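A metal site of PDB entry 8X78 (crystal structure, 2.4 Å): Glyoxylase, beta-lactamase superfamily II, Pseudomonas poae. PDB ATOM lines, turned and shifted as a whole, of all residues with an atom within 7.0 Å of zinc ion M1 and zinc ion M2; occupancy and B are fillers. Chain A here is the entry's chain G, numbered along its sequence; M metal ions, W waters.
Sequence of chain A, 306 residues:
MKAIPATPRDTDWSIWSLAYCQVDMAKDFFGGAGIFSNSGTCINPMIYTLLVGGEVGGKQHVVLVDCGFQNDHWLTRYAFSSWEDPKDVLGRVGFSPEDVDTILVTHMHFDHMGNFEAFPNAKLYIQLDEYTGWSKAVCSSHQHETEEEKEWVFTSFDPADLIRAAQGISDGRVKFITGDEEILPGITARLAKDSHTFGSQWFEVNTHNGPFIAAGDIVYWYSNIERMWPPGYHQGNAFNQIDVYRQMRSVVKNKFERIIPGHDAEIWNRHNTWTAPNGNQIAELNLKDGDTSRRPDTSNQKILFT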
ATOM      1  N   PHE A  30       0.413 -26.999 -10.206  1.00  0.00           N
ATOM      2  CA  PHE A  30       0.645 -25.558 -10.257  1.00  0.00           C
ATOM      3  C   PHE A  30       1.498 -25.021  -9.110  1.00  0.00           C
ATOM      4  O   PHE A  30       2.272 -24.077  -9.308  1.00  0.00           O
ATOM      5  CB  PHE A  30      -0.697 -24.797 -10.238  1.00  0.00           C
ATOM      6  CG  PHE A  30      -1.523 -24.976 -11.489  1.00  0.00           C
ATOM      7  CD1 PHE A  30      -1.003 -24.625 -12.727  1.00  0.00           C
ATOM      8  CD2 PHE A  30      -2.808 -25.481 -11.421  1.00  0.00           C
ATOM      9  CE1 PHE A  30      -1.753 -24.779 -13.884  1.00  0.00           C
ATOM     10  CE2 PHE A  30      -3.573 -25.643 -12.576  1.00  0.00           C
ATOM     11  CZ  PHE A  30      -3.046 -25.292 -13.808  1.00  0.00           C
ATOM     12  N   MET A  46      -8.421 -20.298 -16.883  1.00  0.00           N
ATOM     13  CA  MET A  46      -7.664 -20.091 -18.109  1.00  0.00           C
ATOM     14  C   MET A  46      -7.930 -18.644 -18.505  1.00  0.00           C
ATOM     15  O   MET A  46      -9.088 -18.227 -18.636  1.00  0.00           O
ATOM     16  CB  MET A  46      -8.107 -21.065 -19.206  1.00  0.00           C
ATOM     17  CG  MET A  46      -8.252 -22.503 -18.724  1.00  0.00           C
ATOM     18  SD  MET A  46      -6.717 -23.359 -18.321  1.00  0.00           S
ATOM     19  CE  MET A  46      -5.775 -23.180 -19.829  1.00  0.00           C
ATOM     20  N   ASP A  66      -1.419 -13.308 -24.632  1.00  0.00           N
ATOM     21  CA  ASP A  66      -1.949 -14.654 -24.834  1.00  0.00           C
ATOM     22  C   ASP A  66      -3.379 -14.546 -25.360  1.00  0.00           C
ATOM     23  O   ASP A  66      -3.997 -13.472 -25.308  1.00  0.00           O
ATOM     24  CB  ASP A  66      -1.835 -15.472 -23.538  1.00  0.00           C
ATOM     25  CG  ASP A  66      -0.358 -15.691 -23.091  1.00  0.00           C
ATOM     26  OD1 ASP A  66       0.582 -15.604 -23.941  1.00  0.00           O
ATOM     27  OD2 ASP A  66      -0.118 -15.969 -21.886  1.00  0.00           O
ATOM     28  N   THR A 106       3.309 -15.066 -24.284  1.00  0.00           N
ATOM     29  CA  THR A 106       4.289 -15.391 -23.251  1.00  0.00           C
ATOM     30  C   THR A 106       5.061 -16.648 -23.625  1.00  0.00           C
ATOM     31  O   THR A 106       6.276 -16.729 -23.381  1.00  0.00           O
ATOM     32  CB  THR A 106       3.628 -15.590 -21.880  1.00  0.00           C
ATOM     33  OG1 THR A 106       2.670 -16.644 -21.966  1.00  0.00           O
ATOM     34  CG2 THR A 106       2.938 -14.320 -21.418  1.00  0.00           C
ATOM     35  N   HIS A 107       4.396 -17.636 -24.211  1.00  0.00           N
ATOM     36  CA  HIS A 107       5.018 -18.895 -24.600  1.00  0.00           C
ATOM     37  C   HIS A 107       4.047 -19.634 -25.505  1.00  0.00           C
ATOM     38  O   HIS A 107       2.859 -19.293 -25.559  1.00  0.00           O
ATOM     39  CB  HIS A 107       5.430 -19.768 -23.386  1.00  0.00           C
ATOM     40  CG  HIS A 107       4.291 -20.256 -22.540  1.00  0.00           C
ATOM     41  ND1 HIS A 107       3.378 -19.412 -21.928  1.00  0.00           N
ATOM     42  CD2 HIS A 107       3.979 -21.503 -22.100  1.00  0.00           C
ATOM     43  CE1 HIS A 107       2.548 -20.121 -21.176  1.00  0.00           C
ATOM     44  NE2 HIS A 107       2.880 -21.399 -21.286  1.00  0.00           N
ATOM     45  N   MET A 108       4.548 -20.648 -26.204  1.00  0.00           N
ATOM     46  CA  MET A 108       3.835 -21.306 -27.281  1.00  0.00           C
ATOM     47  C   MET A 108       3.069 -22.539 -26.826  1.00  0.00           C
ATOM     48  O   MET A 108       2.774 -23.402 -27.660  1.00  0.00           O
ATOM     49  CB  MET A 108       4.796 -21.694 -28.413  1.00  0.00           C
ATOM     50  CG  MET A 108       5.154 -20.513 -29.309  1.00  0.00           C
ATOM     51  SD  MET A 108       6.403 -20.862 -30.587  1.00  0.00           S
ATOM     52  CE  MET A 108       5.478 -22.018 -31.639  1.00  0.00           C
ATOM     53  N   HIS A 109       2.781 -22.668 -25.530  1.00  0.00           N
ATOM     54  CA  HIS A 109       1.851 -23.695 -25.078  1.00  0.00           C
ATOM     55  C   HIS A 109       0.453 -23.450 -25.682  1.00  0.00           C
ATOM     56  O   HIS A 109       0.060 -22.306 -25.971  1.00  0.00           O
ATOM     57  CB  HIS A 109       1.815 -23.733 -23.554  1.00  0.00           C
ATOM     58  CG  HIS A 109       2.918 -24.548 -22.940  1.00  0.00           C
ATOM     59  ND1 HIS A 109       3.200 -24.544 -21.593  1.00  0.00           N
ATOM     60  CD2 HIS A 109       3.798 -25.420 -23.504  1.00  0.00           C
ATOM     61  CE1 HIS A 109       4.210 -25.362 -21.347  1.00  0.00           C
ATOM     62  NE2 HIS A 109       4.591 -25.906 -22.490  1.00  0.00           N
ATOM     63  N   PHE A 110      -0.291 -24.541 -25.878  1.00  0.00           N
ATOM     64  CA  PHE A 110      -1.550 -24.460 -26.628  1.00  0.00           C
ATOM     65  C   PHE A 110      -2.510 -23.448 -26.025  1.00  0.00           C
ATOM     66  O   PHE A 110      -3.256 -22.772 -26.754  1.00  0.00           O
ATOM     67  CB  PHE A 110      -2.198 -25.850 -26.691  1.00  0.00           C
ATOM     68  CG  PHE A 110      -2.851 -26.287 -25.399  1.00  0.00           C
ATOM     69  CD1 PHE A 110      -2.074 -26.784 -24.340  1.00  0.00           C
ATOM     70  CD2 PHE A 110      -4.219 -26.227 -25.248  1.00  0.00           C
ATOM     71  CE1 PHE A 110      -2.683 -27.194 -23.169  1.00  0.00           C
ATOM     72  CE2 PHE A 110      -4.842 -26.643 -24.061  1.00  0.00           C
ATOM     73  CZ  PHE A 110      -4.070 -27.122 -23.025  1.00  0.00           C
ATOM     74  N   ASP A 111      -2.550 -23.342 -24.701  1.00  0.00           N
ATOM     75  CA  ASP A 111      -3.534 -22.450 -24.101  1.00  0.00           C
ATOM     76  C   ASP A 111      -3.112 -20.991 -24.061  1.00  0.00           C
ATOM     77  O   ASP A 111      -3.878 -20.157 -23.575  1.00  0.00           O
ATOM     78  CB  ASP A 111      -3.880 -22.953 -22.697  1.00  0.00           C
ATOM     79  CG  ASP A 111      -2.666 -23.111 -21.827  1.00  0.00           C
ATOM     80  OD1 ASP A 111      -1.665 -23.651 -22.315  1.00  0.00           O
ATOM     81  OD2 ASP A 111      -2.724 -22.718 -20.645  1.00  0.00           O
ATOM     82  N   HIS A 112      -1.941 -20.624 -24.604  1.00  0.00           N
ATOM     83  CA  HIS A 112      -1.635 -19.209 -24.689  1.00  0.00           C
ATOM     84  C   HIS A 112      -1.459 -18.697 -26.116  1.00  0.00           C
ATOM     85  O   HIS A 112      -1.599 -17.486 -26.340  1.00  0.00           O
ATOM     86  CB  HIS A 112      -0.369 -18.893 -23.876  1.00  0.00           C
ATOM     87  CG  HIS A 112      -0.521 -19.243 -22.431  1.00  0.00           C
ATOM     88  ND1 HIS A 112      -0.872 -18.312 -21.468  1.00  0.00           N
ATOM     89  CD2 HIS A 112      -0.435 -20.433 -21.787  1.00  0.00           C
ATOM     90  CE1 HIS A 112      -0.965 -18.917 -20.302  1.00  0.00           C
ATOM     91  NE2 HIS A 112      -0.706 -20.193 -20.467  1.00  0.00           N
ATOM     92  N   SER A 156       1.583 -29.943 -23.243  1.00  0.00           N
ATOM     93  CA  SER A 156       1.005 -28.606 -23.440  1.00  0.00           C
ATOM     94  C   SER A 156       1.358 -28.015 -24.793  1.00  0.00           C
ATOM     95  O   SER A 156       1.214 -26.788 -24.982  1.00  0.00           O
ATOM     96  CB  SER A 156       1.478 -27.626 -22.344  1.00  0.00           C
ATOM     97  OG  SER A 156       0.949 -27.990 -21.068  1.00  0.00           O
ATOM     98  N   HIS A 196      10.014 -21.054 -17.687  1.00  0.00           N
ATOM     99  CA  HIS A 196       8.901 -21.982 -17.886  1.00  0.00           C
ATOM    100  C   HIS A 196       9.047 -22.801 -19.173  1.00  0.00           C
ATOM    101  O   HIS A 196       8.658 -23.980 -19.220  1.00  0.00           O
ATOM    102  CB  HIS A 196       7.585 -21.236 -17.881  1.00  0.00           C
ATOM    103  CG  HIS A 196       6.404 -22.153 -17.936  1.00  0.00           C
ATOM    104  ND1 HIS A 196       5.549 -22.208 -19.010  1.00  0.00           N
ATOM    105  CD2 HIS A 196       5.974 -23.081 -17.052  1.00  0.00           C
ATOM    106  CE1 HIS A 196       4.624 -23.117 -18.783  1.00  0.00           C
ATOM    107  NE2 HIS A 196       4.854 -23.662 -17.595  1.00  0.00           N
ATOM    108  N   THR A 197       9.572 -22.190 -20.242  1.00  0.00           N
ATOM    109  CA  THR A 197       9.813 -22.847 -21.513  1.00  0.00           C
ATOM    110  C   THR A 197      11.056 -22.216 -22.134  1.00  0.00           C
ATOM    111  O   THR A 197      11.596 -21.241 -21.605  1.00  0.00           O
ATOM    112  CB  THR A 197       8.628 -22.719 -22.488  1.00  0.00           C
ATOM    113  OG1 THR A 197       8.439 -21.339 -22.849  1.00  0.00           O
ATOM    114  CG2 THR A 197       7.379 -23.199 -21.818  1.00  0.00           C
ATOM    115  N   SER A 200      10.112 -18.455 -22.832  1.00  0.00           N
ATOM    116  CA  SER A 200       9.063 -17.732 -22.132  1.00  0.00           C
ATOM    117  C   SER A 200       9.479 -16.271 -22.014  1.00  0.00           C
ATOM    118  O   SER A 200      10.668 -15.971 -21.847  1.00  0.00           O
ATOM    119  CB  SER A 200       8.841 -18.314 -20.729  1.00  0.00           C
ATOM    120  OG  SER A 200       8.032 -19.481 -20.754  1.00  0.00           O
ATOM    121  N   GLY A 216       2.829 -14.774 -17.542  1.00  0.00           N
ATOM    122  CA  GLY A 216       2.680 -16.042 -18.221  1.00  0.00           C
ATOM    123  C   GLY A 216       2.659 -17.172 -17.217  1.00  0.00           C
ATOM    124  O   GLY A 216       2.207 -17.025 -16.069  1.00  0.00           O
ATOM    125  N   ASP A 217       3.154 -18.315 -17.632  1.00  0.00           N
ATOM    126  CA  ASP A 217       3.214 -19.464 -16.742  1.00  0.00           C
ATOM    127  C   ASP A 217       4.498 -19.526 -15.918  1.00  0.00           C
ATOM    128  O   ASP A 217       4.683 -20.488 -15.161  1.00  0.00           O
ATOM    129  CB  ASP A 217       3.075 -20.750 -17.534  1.00  0.00           C
ATOM    130  CG  ASP A 217       1.648 -21.043 -17.872  1.00  0.00           C
ATOM    131  OD1 ASP A 217       0.763 -20.294 -17.390  1.00  0.00           O
ATOM    132  OD2 ASP A 217       1.435 -21.997 -18.631  1.00  0.00           O
ATOM    133  N   ILE A 218       5.386 -18.538 -16.062  1.00  0.00           N
ATOM    134  CA  ILE A 218       6.478 -18.411 -15.108  1.00  0.00           C
ATOM    135  C   ILE A 218       5.926 -18.353 -13.693  1.00  0.00           C
ATOM    136  O   ILE A 218       6.445 -18.988 -12.768  1.00  0.00           O
ATOM    137  CB  ILE A 218       7.331 -17.186 -15.465  1.00  0.00           C
ATOM    138  CG1 ILE A 218       7.958 -17.373 -16.856  1.00  0.00           C
ATOM    139  CG2 ILE A 218       8.410 -16.964 -14.438  1.00  0.00           C
ATOM    140  CD1 ILE A 218       8.649 -16.163 -17.391  1.00  0.00           C
ATOM    141  N   TYR A 220       2.566 -19.514 -12.254  1.00  0.00           N
ATOM    142  CA  TYR A 220       1.249 -20.132 -12.283  1.00  0.00           C
ATOM    143  C   TYR A 220       0.340 -19.526 -11.221  1.00  0.00           C
ATOM    144  O   TYR A 220      -0.797 -19.144 -11.491  1.00  0.00           O
ATOM    145  CB  TYR A 220       1.384 -21.630 -12.010  1.00  0.00           C
ATOM    146  CG  TYR A 220       1.690 -22.553 -13.159  1.00  0.00           C
ATOM    147  CD1 TYR A 220       1.184 -22.338 -14.415  1.00  0.00           C
ATOM    148  CD2 TYR A 220       2.477 -23.683 -12.951  1.00  0.00           C
ATOM    149  CE1 TYR A 220       1.453 -23.229 -15.453  1.00  0.00           C
ATOM    150  CE2 TYR A 220       2.754 -24.571 -13.968  1.00  0.00           C
ATOM    151  CZ  TYR A 220       2.236 -24.342 -15.212  1.00  0.00           C
ATOM    152  OH  TYR A 220       2.527 -25.233 -16.229  1.00  0.00           O
ATOM    153  N   TYR A 233       4.921 -28.830 -12.407  1.00  0.00           N
ATOM    154  CA  TYR A 233       4.983 -29.018 -13.841  1.00  0.00           C
ATOM    155  C   TYR A 233       5.470 -27.721 -14.466  1.00  0.00           C
ATOM    156  O   TYR A 233       4.919 -26.653 -14.195  1.00  0.00           O
ATOM    157  CB  TYR A 233       3.622 -29.420 -14.437  1.00  0.00           C
ATOM    158  CG  TYR A 233       3.641 -29.400 -15.957  1.00  0.00           C
ATOM    159  CD1 TYR A 233       4.146 -30.479 -16.676  1.00  0.00           C
ATOM    160  CD2 TYR A 233       3.222 -28.287 -16.670  1.00  0.00           C
ATOM    161  CE1 TYR A 233       4.217 -30.464 -18.047  1.00  0.00           C
ATOM    162  CE2 TYR A 233       3.267 -28.248 -18.044  1.00  0.00           C
ATOM    163  CZ  TYR A 233       3.771 -29.342 -18.732  1.00  0.00           C
ATOM    164  OH  TYR A 233       3.815 -29.313 -20.104  1.00  0.00           O
ATOM    165  N   GLN A 235       8.439 -26.681 -18.054  1.00  0.00           N
ATOM    166  CA  GLN A 235       9.317 -27.263 -19.054  1.00  0.00           C
ATOM    167  C   GLN A 235      10.598 -26.468 -19.235  1.00  0.00           C
ATOM    168  O   GLN A 235      11.100 -26.310 -20.351  1.00  0.00           O
ATOM    169  CB  GLN A 235       8.567 -27.452 -20.370  1.00  0.00           C
ATOM    170  CG  GLN A 235       7.312 -28.317 -20.158  1.00  0.00           C
ATOM    171  CD  GLN A 235       6.703 -28.820 -21.462  1.00  0.00           C
ATOM    172  OE1 GLN A 235       6.177 -28.043 -22.265  1.00  0.00           O
ATOM    173  NE2 GLN A 235       6.749 -30.134 -21.663  1.00  0.00           N
ATOM    174  N   GLY A 262      -0.658 -17.021 -14.170  1.00  0.00           N
ATOM    175  CA  GLY A 262      -1.249 -17.668 -15.332  1.00  0.00           C
ATOM    176  C   GLY A 262      -2.576 -18.348 -15.044  1.00  0.00           C
ATOM    177  O   GLY A 262      -3.500 -18.262 -15.858  1.00  0.00           O
ATOM    178  N   HIS A 263      -2.701 -19.022 -13.888  1.00  0.00           N
ATOM    179  CA  HIS A 263      -3.808 -19.952 -13.701  1.00  0.00           C
ATOM    180  C   HIS A 263      -4.255 -20.013 -12.237  1.00  0.00           C
ATOM    181  O   HIS A 263      -4.533 -21.085 -11.689  1.00  0.00           O
ATOM    182  CB  HIS A 263      -3.407 -21.341 -14.205  1.00  0.00           C
ATOM    183  CG  HIS A 263      -3.167 -21.376 -15.683  1.00  0.00           C
ATOM    184  ND1 HIS A 263      -4.160 -21.113 -16.599  1.00  0.00           N
ATOM    185  CD2 HIS A 263      -2.037 -21.579 -16.384  1.00  0.00           C
ATOM    186  CE1 HIS A 263      -3.656 -21.185 -17.817  1.00  0.00           C
ATOM    187  NE2 HIS A 263      -2.372 -21.461 -17.718  1.00  0.00           N
HETATM  188 ZN    ZN M   1      -0.832 -22.092 -19.244  1.00  0.00          ZN
HETATM  189 ZN    ZN M   2       2.326 -23.254 -19.961  1.00  0.00          ZN
HETATM  190  O   HOH W   1      -0.341 -23.808 -20.133  1.00  0.00           O
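Within 4 Å of zinc ion M1: Asp 111, His 112, Asp 217 and His 263.
Zinc ion M1 is bound by water W1 (2.0 Å), NE2 of His 263 (2.3 Å), NE2 of His 112 (2.3 Å), OD2 of Asp 217 (2.4 Å) and OD2 of Asp 111 (2.4 Å). Zinc ion M1 has five donor atoms within binding distance.
OD2 of Asp 217 is bound to zinc ion M2, at 2.0 Å. Zinc ion M2 is bound by a ring nitrogen (ND1) of His 109. NE2 of His 107 is bound to zinc ion M2 (2.3 Å). Slightly farther from zinc ion M2 lies water W1 (2.7 Å).
A ring nitrogen (NE2) of His 109 is in hydrogen-bond range of the side-chain amide oxygen of Gln 235 (2.7 Å). The backbone NH (N) of His 263 sits at hydrogen-bond distance from the backbone carbonyl oxygen (O) of Tyr 220, 3.1 Å away. The side-chain carboxylate (OD2) of Asp 66 sits at hydrogen-bond distance from a ring nitrogen (ND1) of His 112. The side-chain hydroxyl of Thr 106 lies within hydrogen-bond range of a ring nitrogen (ND1) of His 107, 2.9 Å away. The side-chain hydroxyl of Tyr 220 lies within hydrogen-bond range of a ring nitrogen (NE2) of His 196, at 3.1 Å. N of Gln 235 is in hydrogen-bond range of O of His 196, 3.0 Å away.
Merely in contact with zinc ion M2: His 196. Of the 22 residues printed, 4 come within 4 Å of zinc ion M2.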
